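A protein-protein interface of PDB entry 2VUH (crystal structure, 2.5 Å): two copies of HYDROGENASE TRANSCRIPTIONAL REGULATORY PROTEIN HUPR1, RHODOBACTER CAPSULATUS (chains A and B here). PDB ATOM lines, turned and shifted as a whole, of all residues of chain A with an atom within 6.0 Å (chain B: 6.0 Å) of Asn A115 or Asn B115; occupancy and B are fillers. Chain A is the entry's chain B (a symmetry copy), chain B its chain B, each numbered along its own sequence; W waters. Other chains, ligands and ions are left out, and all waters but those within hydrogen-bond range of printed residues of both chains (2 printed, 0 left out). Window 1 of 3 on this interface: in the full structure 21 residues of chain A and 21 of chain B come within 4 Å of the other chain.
ND2 of Asn A115 lies within hydrogen-bond range of O of His B97 (3.0 Å). ND2 of Asn B115 sits at hydrogen-bond distance from O of His A97 (3.0 Å). The side-chain amide oxygen of Asn B115 lies close to the side-chain amide oxygen of Asn A115 (2.9 Å). The guanidinium group (NH2) of Arg B118 is in hydrogen-bond range of the backbone carbonyl oxygen (O) of His A97 (3.1 Å). The backbone carbonyl oxygen of His B97 lies within hydrogen-bond range of the guanidinium group of Arg A118.
The side-chain amide nitrogen (NE2) of Gln B98 lies within hydrogen-bond range of the side-chain amide oxygen (OD1) of Asn B115 (3.2 Å). The side-chain amide oxygen of Gln B98 sits at hydrogen-bond distance from the side-chain hydroxyl of Ser B112 (2.7 Å). The side-chain amide oxygen (OE1) of Gln A98 lies within hydrogen-bond range of the side-chain hydroxyl (OG) of Ser A112 (2.7 Å). The side-chain amide nitrogen (NE2) of Gln A98 is in hydrogen-bond range of the side-chain amide oxygen (OD1) of Asn A115 (3.2 Å).
Among the printed residues, merely in contact across the chains: His A97 with Ser B111, Gln A98 with Ser B111, Gln A98 with Asn B115, Ser A111 with His B97, Ser A111 with Gln B98, Asn A115 with Gln B98 and Met A119 with Met B119.
Asn A115 touches just these residues of chain B: His B97 (3.0 Å), Gln B98 (3.8 Å) and Asn B115 (2.9 Å). Ala A116 touches none of the printed residues of chain B. Printed residues of chain B within 4 Å of Met A119: Met B119 (3.8 Å). Printed residues of chain A within 4 Å of Ser B111: His A97 (3.997 Å) and Gln A98 (3.4 Å). Arg B114 touches none of the printed residues of chain A. Asn B115 touches three residues of chain A. The nearest residue of chain A that does not touch Asn B115 is Met A119 (4.02 Å).
Printed residues of chain B that touch a printed residue of chain A: His B97, Gln B98, Ser B111, Asn B115, Arg B118 and Met B119. Of the 14 printed residues of chain A, 6 touch a printed residue of chain B. Printed residues of chain A that touch a printed residue of chain B: His A97, Gln A98, Ser A111, Asn A115, Arg A118 and Met A119. Hydrophobic or aromatic side chains of chain A within 4 Å of the printed part of chain B: His A97 and Met A119. Among the printed residues, no Asp or Glu carboxylate lies within 4 Å of a Lys or Arg side-chain nitrogen of the other chain.
His A97 touches Ser B111, and with the chains exchanged Ser A111 touches His B97. His A97 touches Asn B115, and with the chains exchanged Asn A115 touches His B97. Asn B115 touches its own counterpart, Asn A115. Met A119 touches its own counterpart, Met B119. Positions printed for both chains: 74, 97, 98, 110, 111, 112, 113, 114, 115, 116, 117, 118, 119 and 120.
Water W2 lies within hydrogen-bond range of the backbone carbonyl oxygen of Ser A111 (3.0 Å), the backbone carbonyl oxygen of His B97 (3.0 Å) and the guanidinium group of Arg A118 (3.2 Å). Water W1 lies within hydrogen-bond range of the backbone carbonyl oxygen (O) of Ser B111 (3.0 Å), the backbone carbonyl oxygen (O) of His A97 (3.0 Å) and the guanidinium group (NH2) of Arg B118 (3.2 Å).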
ATOM      1  N   VAL A  74     -23.611 -21.422  -0.588  1.00  0.00           N
ATOM      2  CA  VAL A  74     -24.704 -20.497  -0.865  1.00  0.00           C
ATOM      3  C   VAL A  74     -24.957 -20.508  -2.379  1.00  0.00           C
ATOM      4  O   VAL A  74     -24.011 -20.377  -3.155  1.00  0.00           O
ATOM      5  CB  VAL A  74     -24.374 -19.089  -0.321  1.00  0.00           C
ATOM      6  CG1 VAL A  74     -25.501 -18.110  -0.652  1.00  0.00           C
ATOM      7  CG2 VAL A  74     -24.127 -19.155   1.195  1.00  0.00           C
ATOM      8  N   HIS A  97     -30.749 -19.123  -2.655  1.00  0.00           N
ATOM      9  CA  HIS A  97     -30.570 -17.968  -1.797  1.00  0.00           C
ATOM     10  C   HIS A  97     -30.720 -16.600  -2.481  1.00  0.00           C
ATOM     11  O   HIS A  97     -31.111 -15.613  -1.821  1.00  0.00           O
ATOM     12  CB  HIS A  97     -29.241 -18.102  -1.049  1.00  0.00           C
ATOM     13  CG  HIS A  97     -29.030 -19.486  -0.496  1.00  0.00           C
ATOM     14  ND1 HIS A  97     -28.413 -20.497  -1.215  1.00  0.00           N
ATOM     15  CD2 HIS A  97     -29.415 -20.044   0.681  1.00  0.00           C
ATOM     16  CE1 HIS A  97     -28.401 -21.602  -0.497  1.00  0.00           C
ATOM     17  NE2 HIS A  97     -29.004 -21.356   0.654  1.00  0.00           N
ATOM     18  N   GLN A  98     -30.381 -16.526  -3.773  1.00  0.00           N
ATOM     19  CA  GLN A  98     -30.590 -15.308  -4.560  1.00  0.00           C
ATOM     20  C   GLN A  98     -30.905 -15.623  -5.990  1.00  0.00           C
ATOM     21  O   GLN A  98     -30.364 -16.576  -6.594  1.00  0.00           O
ATOM     22  CB  GLN A  98     -29.409 -14.335  -4.526  1.00  0.00           C
ATOM     23  CG  GLN A  98     -28.733 -14.163  -3.140  1.00  0.00           C
ATOM     24  CD  GLN A  98     -28.042 -12.810  -3.001  1.00  0.00           C
ATOM     25  OE1 GLN A  98     -28.495 -11.817  -3.612  1.00  0.00           O
ATOM     26  NE2 GLN A  98     -26.952 -12.750  -2.191  1.00  0.00           N
ATOM     27  N   LEU A 110     -21.117  -7.875  -7.495  1.00  0.00           N
ATOM     28  CA  LEU A 110     -20.147  -7.936  -6.423  1.00  0.00           C
ATOM     29  C   LEU A 110     -20.837  -7.910  -5.058  1.00  0.00           C
ATOM     30  O   LEU A 110     -20.548  -8.769  -4.209  1.00  0.00           O
ATOM     31  CB  LEU A 110     -19.156  -6.780  -6.549  1.00  0.00           C
ATOM     32  CG  LEU A 110     -18.159  -6.682  -5.404  1.00  0.00           C
ATOM     33  CD1 LEU A 110     -17.339  -7.978  -5.230  1.00  0.00           C
ATOM     34  CD2 LEU A 110     -17.255  -5.470  -5.663  1.00  0.00           C
ATOM     35  N   SER A 111     -21.782  -6.981  -4.860  1.00  0.00           N
ATOM     36  CA  SER A 111     -22.476  -6.893  -3.581  1.00  0.00           C
ATOM     37  C   SER A 111     -23.253  -8.163  -3.236  1.00  0.00           C
ATOM     38  O   SER A 111     -23.286  -8.601  -2.079  1.00  0.00           O
ATOM     39  CB  SER A 111     -23.428  -5.684  -3.561  1.00  0.00           C
ATOM     40  OG  SER A 111     -24.131  -5.579  -2.327  1.00  0.00           O
ATOM     41  N   SER A 112     -23.926  -8.735  -4.220  1.00  0.00           N
ATOM     42  CA  SER A 112     -24.596 -10.021  -4.012  1.00  0.00           C
ATOM     43  C   SER A 112     -23.634 -11.131  -3.589  1.00  0.00           C
ATOM     44  O   SER A 112     -23.943 -11.935  -2.702  1.00  0.00           O
ATOM     45  CB  SER A 112     -25.220 -10.465  -5.304  1.00  0.00           C
ATOM     46  OG  SER A 112     -26.603 -10.569  -5.143  1.00  0.00           O
ATOM     47  N   ALA A 113     -22.484 -11.186  -4.256  1.00  0.00           N
ATOM     48  CA  ALA A 113     -21.509 -12.178  -3.974  1.00  0.00           C
ATOM     49  C   ALA A 113     -21.027 -11.982  -2.529  1.00  0.00           C
ATOM     50  O   ALA A 113     -21.079 -12.926  -1.725  1.00  0.00           O
ATOM     51  CB  ALA A 113     -20.348 -12.094  -5.009  1.00  0.00           C
ATOM     52  N   ARG A 114     -20.566 -10.777  -2.175  1.00  0.00           N
ATOM     53  CA  ARG A 114     -20.033 -10.514  -0.802  1.00  0.00           C
ATOM     54  C   ARG A 114     -21.014 -10.880   0.294  1.00  0.00           C
ATOM     55  O   ARG A 114     -20.621 -11.367   1.371  1.00  0.00           O
ATOM     56  CB  ARG A 114     -19.697  -9.049  -0.595  1.00  0.00           C
ATOM     57  CG  ARG A 114     -18.455  -8.518  -1.293  1.00  0.00           C
ATOM     58  CD  ARG A 114     -18.429  -7.006  -1.102  1.00  0.00           C
ATOM     59  NE  ARG A 114     -17.129  -6.432  -1.437  1.00  0.00           N
ATOM     60  CZ  ARG A 114     -16.956  -5.202  -1.940  1.00  0.00           C
ATOM     61  NH1 ARG A 114     -18.027  -4.436  -2.177  1.00  0.00           N
ATOM     62  NH2 ARG A 114     -15.726  -4.730  -2.211  1.00  0.00           N
ATOM     63  N   ASN A 115     -22.276 -10.618   0.001  1.00  0.00           N
ATOM     64  CA  ASN A 115     -23.404 -10.844   0.865  1.00  0.00           C
ATOM     65  C   ASN A 115     -23.727 -12.351   1.059  1.00  0.00           C
ATOM     66  O   ASN A 115     -24.045 -12.817   2.176  1.00  0.00           O
ATOM     67  CB  ASN A 115     -24.587 -10.093   0.236  1.00  0.00           C
ATOM     68  CG  ASN A 115     -25.853 -10.300   0.976  1.00  0.00           C
ATOM     69  OD1 ASN A 115     -26.658 -11.143   0.579  1.00  0.00           O
ATOM     70  ND2 ASN A 115     -26.041  -9.568   2.111  1.00  0.00           N
ATOM     71  N   ALA A 116     -23.664 -13.099  -0.044  1.00  0.00           N
ATOM     72  CA  ALA A 116     -23.637 -14.561  -0.025  1.00  0.00           C
ATOM     73  C   ALA A 116     -22.456 -15.131   0.761  1.00  0.00           C
ATOM     74  O   ALA A 116     -22.615 -16.079   1.498  1.00  0.00           O
ATOM     75  CB  ALA A 116     -23.616 -15.080  -1.437  1.00  0.00           C
ATOM     76  N   ALA A 117     -21.271 -14.575   0.587  1.00  0.00           N
ATOM     77  CA  ALA A 117     -20.122 -15.015   1.372  1.00  0.00           C
ATOM     78  C   ALA A 117     -20.356 -14.789   2.888  1.00  0.00           C
ATOM     79  O   ALA A 117     -20.128 -15.699   3.708  1.00  0.00           O
ATOM     80  CB  ALA A 117     -18.852 -14.314   0.914  1.00  0.00           C
ATOM     81  N   ARG A 118     -20.839 -13.600   3.259  1.00  0.00           N
ATOM     82  CA  ARG A 118     -21.084 -13.314   4.668  1.00  0.00           C
ATOM     83  C   ARG A 118     -22.137 -14.243   5.186  1.00  0.00           C
ATOM     84  O   ARG A 118     -22.104 -14.660   6.341  1.00  0.00           O
ATOM     85  CB  ARG A 118     -21.457 -11.848   4.937  1.00  0.00           C
ATOM     86  CG  ARG A 118     -20.201 -10.931   4.887  1.00  0.00           C
ATOM     87  CD  ARG A 118     -20.498  -9.445   5.237  1.00  0.00           C
ATOM     88  NE  ARG A 118     -21.797  -9.010   4.693  1.00  0.00           N
ATOM     89  CZ  ARG A 118     -21.965  -8.157   3.684  1.00  0.00           C
ATOM     90  NH1 ARG A 118     -20.914  -7.590   3.082  1.00  0.00           N
ATOM     91  NH2 ARG A 118     -23.204  -7.870   3.291  1.00  0.00           N
ATOM     92  N   MET A 119     -23.062 -14.618   4.332  1.00  0.00           N
ATOM     93  CA  MET A 119     -24.075 -15.524   4.797  1.00  0.00           C
ATOM     94  C   MET A 119     -23.535 -16.953   4.978  1.00  0.00           C
ATOM     95  O   MET A 119     -23.966 -17.709   5.859  1.00  0.00           O
ATOM     96  CB  MET A 119     -25.216 -15.517   3.839  1.00  0.00           C
ATOM     97  CG  MET A 119     -25.861 -16.796   3.874  1.00  0.00           C
ATOM     98  SD  MET A 119     -27.554 -16.633   3.402  1.00  0.00           S
ATOM     99  CE  MET A 119     -28.200 -15.380   4.611  1.00  0.00           C
ATOM    100  N   PHE A 120     -22.573 -17.309   4.142  1.00  0.00           N
ATOM    101  CA  PHE A 120     -21.951 -18.602   4.240  1.00  0.00           C
ATOM    102  C   PHE A 120     -21.270 -18.689   5.584  1.00  0.00           C
ATOM    103  O   PHE A 120     -21.423 -19.671   6.289  1.00  0.00           O
ATOM    104  CB  PHE A 120     -20.929 -18.747   3.120  1.00  0.00           C
ATOM    105  CG  PHE A 120     -19.983 -19.877   3.304  1.00  0.00           C
ATOM    106  CD1 PHE A 120     -20.341 -21.162   2.915  1.00  0.00           C
ATOM    107  CD2 PHE A 120     -18.729 -19.654   3.840  1.00  0.00           C
ATOM    108  CE1 PHE A 120     -19.466 -22.217   3.062  1.00  0.00           C
ATOM    109  CE2 PHE A 120     -17.842 -20.692   4.003  1.00  0.00           C
ATOM    110  CZ  PHE A 120     -18.208 -21.986   3.604  1.00  0.00           C
ATOM    111  N   VAL B  74     -30.980  -5.249   8.883  1.00  0.00           N
ATOM    112  CA  VAL B  74     -30.203  -5.442   7.664  1.00  0.00           C
ATOM    113  C   VAL B  74     -30.466  -4.241   6.745  1.00  0.00           C
ATOM    114  O   VAL B  74     -31.623  -3.884   6.524  1.00  0.00           O
ATOM    115  CB  VAL B  74     -30.558  -6.792   7.003  1.00  0.00           C
ATOM    116  CG1 VAL B  74     -29.776  -6.973   5.702  1.00  0.00           C
ATOM    117  CG2 VAL B  74     -30.277  -7.946   7.980  1.00  0.00           C
ATOM    118  N   HIS B  97     -25.392  -3.964   3.626  1.00  0.00           N
ATOM    119  CA  HIS B  97     -25.462  -5.372   3.284  1.00  0.00           C
ATOM    120  C   HIS B  97     -25.768  -5.685   1.810  1.00  0.00           C
ATOM    121  O   HIS B  97     -25.346  -6.744   1.298  1.00  0.00           O
ATOM    122  CB  HIS B  97     -26.430  -6.072   4.241  1.00  0.00           C
ATOM    123  CG  HIS B  97     -26.221  -5.659   5.673  1.00  0.00           C
ATOM    124  ND1 HIS B  97     -26.869  -4.576   6.245  1.00  0.00           N
ATOM    125  CD2 HIS B  97     -25.385  -6.144   6.627  1.00  0.00           C
ATOM    126  CE1 HIS B  97     -26.465  -4.433   7.492  1.00  0.00           C
ATOM    127  NE2 HIS B  97     -25.565  -5.367   7.747  1.00  0.00           N
ATOM    128  N   GLN B  98     -26.522  -4.802   1.145  1.00  0.00           N
ATOM    129  CA  GLN B  98     -26.783  -4.932  -0.290  1.00  0.00           C
ATOM    130  C   GLN B  98     -26.910  -3.595  -0.951  1.00  0.00           C
ATOM    131  O   GLN B  98     -27.459  -2.623  -0.383  1.00  0.00           O
ATOM    132  CB  GLN B  98     -28.027  -5.759  -0.623  1.00  0.00           C
ATOM    133  CG  GLN B  98     -28.227  -7.032   0.242  1.00  0.00           C
ATOM    134  CD  GLN B  98     -29.042  -8.098  -0.484  1.00  0.00           C
ATOM    135  OE1 GLN B  98     -28.982  -8.182  -1.731  1.00  0.00           O
ATOM    136  NE2 GLN B  98     -29.799  -8.928   0.281  1.00  0.00           N
ATOM    137  N   LEU B 110     -37.761  -8.886  -4.467  1.00  0.00           N
ATOM    138  CA  LEU B 110     -38.300  -9.822  -3.503  1.00  0.00           C
ATOM    139  C   LEU B 110     -37.213 -10.766  -2.989  1.00  0.00           C
ATOM    140  O   LEU B 110     -37.063 -10.921  -1.765  1.00  0.00           O
ATOM    141  CB  LEU B 110     -39.450 -10.611  -4.126  1.00  0.00           C
ATOM    142  CG  LEU B 110     -40.016 -11.705  -3.235  1.00  0.00           C
ATOM    143  CD1 LEU B 110     -40.512 -11.157  -1.880  1.00  0.00           C
ATOM    144  CD2 LEU B 110     -41.138 -12.414  -4.004  1.00  0.00           C
ATOM    145  N   SER B 111     -36.418 -11.348  -3.898  1.00  0.00           N
ATOM    146  CA  SER B 111     -35.365 -12.265  -3.481  1.00  0.00           C
ATOM    147  C   SER B 111     -34.324 -11.606  -2.577  1.00  0.00           C
ATOM    148  O   SER B 111     -33.841 -12.207  -1.609  1.00  0.00           O
ATOM    149  CB  SER B 111     -34.668 -12.885  -4.704  1.00  0.00           C
ATOM    150  OG  SER B 111     -33.624 -13.778  -4.329  1.00  0.00           O
ATOM    151  N   SER B 112     -33.930 -10.389  -2.912  1.00  0.00           N
ATOM    152  CA  SER B 112     -33.031  -9.633  -2.036  1.00  0.00           C
ATOM    153  C   SER B 112     -33.607  -9.414  -0.638  1.00  0.00           C
ATOM    154  O   SER B 112     -32.897  -9.535   0.367  1.00  0.00           O
ATOM    155  CB  SER B 112     -32.805  -8.269  -2.624  1.00  0.00           C
ATOM    156  OG  SER B 112     -31.448  -8.104  -2.911  1.00  0.00           O
ATOM    157  N   ALA B 113     -34.888  -9.057  -0.589  1.00  0.00           N
ATOM    158  CA  ALA B 113     -35.542  -8.806   0.645  1.00  0.00           C
ATOM    159  C   ALA B 113     -35.546 -10.108   1.461  1.00  0.00           C
ATOM    160  O   ALA B 113     -35.080 -10.121   2.611  1.00  0.00           O
ATOM    161  CB  ALA B 113     -36.977  -8.258   0.387  1.00  0.00           C
ATOM    162  N   ARG B 114     -36.052 -11.208   0.893  1.00  0.00           N
ATOM    163  CA  ARG B 114     -36.138 -12.505   1.633  1.00  0.00           C
ATOM    164  C   ARG B 114     -34.805 -12.953   2.200  1.00  0.00           C
ATOM    165  O   ARG B 114     -34.737 -13.531   3.301  1.00  0.00           O
ATOM    166  CB  ARG B 114     -36.618 -13.636   0.743  1.00  0.00           C
ATOM    167  CG  ARG B 114     -38.089 -13.638   0.359  1.00  0.00           C
ATOM    168  CD  ARG B 114     -38.294 -14.735  -0.678  1.00  0.00           C
ATOM    169  NE  ARG B 114     -39.706 -15.051  -0.873  1.00  0.00           N
ATOM    170  CZ  ARG B 114     -40.232 -15.466  -2.035  1.00  0.00           C
ATOM    171  NH1 ARG B 114     -39.436 -15.594  -3.103  1.00  0.00           N
ATOM    172  NH2 ARG B 114     -41.541 -15.754  -2.140  1.00  0.00           N
ATOM    173  N   ASN B 115     -33.769 -12.690   1.421  1.00  0.00           N
ATOM    174  CA  ASN B 115     -32.399 -13.024   1.703  1.00  0.00           C
ATOM    175  C   ASN B 115     -31.792 -12.175   2.852  1.00  0.00           C
ATOM    176  O   ASN B 115     -31.052 -12.682   3.724  1.00  0.00           O
ATOM    177  CB  ASN B 115     -31.628 -12.825   0.389  1.00  0.00           C
ATOM    178  CG  ASN B 115     -30.172 -13.055   0.543  1.00  0.00           C
ATOM    179  OD1 ASN B 115     -29.418 -12.094   0.698  1.00  0.00           O
ATOM    180  ND2 ASN B 115     -29.741 -14.349   0.555  1.00  0.00           N
ATOM    181  N   ALA B 116     -32.094 -10.875   2.827  1.00  0.00           N
ATOM    182  CA  ALA B 116     -31.877  -9.977   3.962  1.00  0.00           C
ATOM    183  C   ALA B 116     -32.624 -10.409   5.223  1.00  0.00           C
ATOM    184  O   ALA B 116     -32.080 -10.350   6.304  1.00  0.00           O
ATOM    185  CB  ALA B 116     -32.277  -8.579   3.577  1.00  0.00           C
ATOM    186  N   ALA B 117     -33.873 -10.816   5.094  1.00  0.00           N
ATOM    187  CA  ALA B 117     -34.612 -11.324   6.245  1.00  0.00           C
ATOM    188  C   ALA B 117     -33.931 -12.583   6.840  1.00  0.00           C
ATOM    189  O   ALA B 117     -33.726 -12.673   8.066  1.00  0.00           O
ATOM    190  CB  ALA B 117     -36.057 -11.620   5.874  1.00  0.00           C
ATOM    191  N   ARG B 118     -33.552 -13.534   5.982  1.00  0.00           N
ATOM    192  CA  ARG B 118     -32.905 -14.747   6.470  1.00  0.00           C
ATOM    193  C   ARG B 118     -31.605 -14.389   7.118  1.00  0.00           C
ATOM    194  O   ARG B 118     -31.187 -15.013   8.091  1.00  0.00           O
ATOM    195  CB  ARG B 118     -32.706 -15.811   5.379  1.00  0.00           C
ATOM    196  CG  ARG B 118     -34.039 -16.551   5.068  1.00  0.00           C
ATOM    197  CD  ARG B 118     -33.887 -17.701   4.032  1.00  0.00           C
ATOM    198  NE  ARG B 118     -32.928 -17.350   2.969  1.00  0.00           N
ATOM    199  CZ  ARG B 118     -33.241 -17.090   1.701  1.00  0.00           C
ATOM    200  NH1 ARG B 118     -34.509 -17.156   1.280  1.00  0.00           N
ATOM    201  NH2 ARG B 118     -32.264 -16.770   0.855  1.00  0.00           N
ATOM    202  N   MET B 119     -30.965 -13.354   6.624  1.00  0.00           N
ATOM    203  CA  MET B 119     -29.724 -12.977   7.240  1.00  0.00           C
ATOM    204  C   MET B 119     -29.936 -12.305   8.606  1.00  0.00           C
ATOM    205  O   MET B 119     -29.123 -12.432   9.531  1.00  0.00           O
ATOM    206  CB  MET B 119     -28.979 -12.067   6.323  1.00  0.00           C
ATOM    207  CG  MET B 119     -28.162 -11.187   7.105  1.00  0.00           C
ATOM    208  SD  MET B 119     -26.769 -10.657   6.159  1.00  0.00           S
ATOM    209  CE  MET B 119     -25.972 -12.260   5.665  1.00  0.00           C
ATOM    210  N   PHE B 120     -31.049 -11.599   8.729  1.00  0.00           N
ATOM    211  CA  PHE B 120     -31.387 -10.964   9.974  1.00  0.00           C
ATOM    212  C   PHE B 120     -31.564 -12.044  11.014  1.00  0.00           C
ATOM    213  O   PHE B 120     -31.030 -11.939  12.105  1.00  0.00           O
ATOM    214  CB  PHE B 120     -32.683 -10.184   9.797  1.00  0.00           C
ATOM    215  CG  PHE B 120     -33.321  -9.768  11.072  1.00  0.00           C
ATOM    216  CD1 PHE B 120     -32.909  -8.608  11.717  1.00  0.00           C
ATOM    217  CD2 PHE B 120     -34.346 -10.518  11.614  1.00  0.00           C
ATOM    218  CE1 PHE B 120     -33.504  -8.199  12.890  1.00  0.00           C
ATOM    219  CE2 PHE B 120     -34.950 -10.135  12.789  1.00  0.00           C
ATOM    220  CZ  PHE B 120     -34.533  -8.961  13.432  1.00  0.00           C
HETATM  221  O   HOH W   1     -34.053 -15.179  -1.310  1.00  0.00           O
HETATM  222  O   HOH W   2     -22.511  -6.931   0.281  1.00  0.00           O
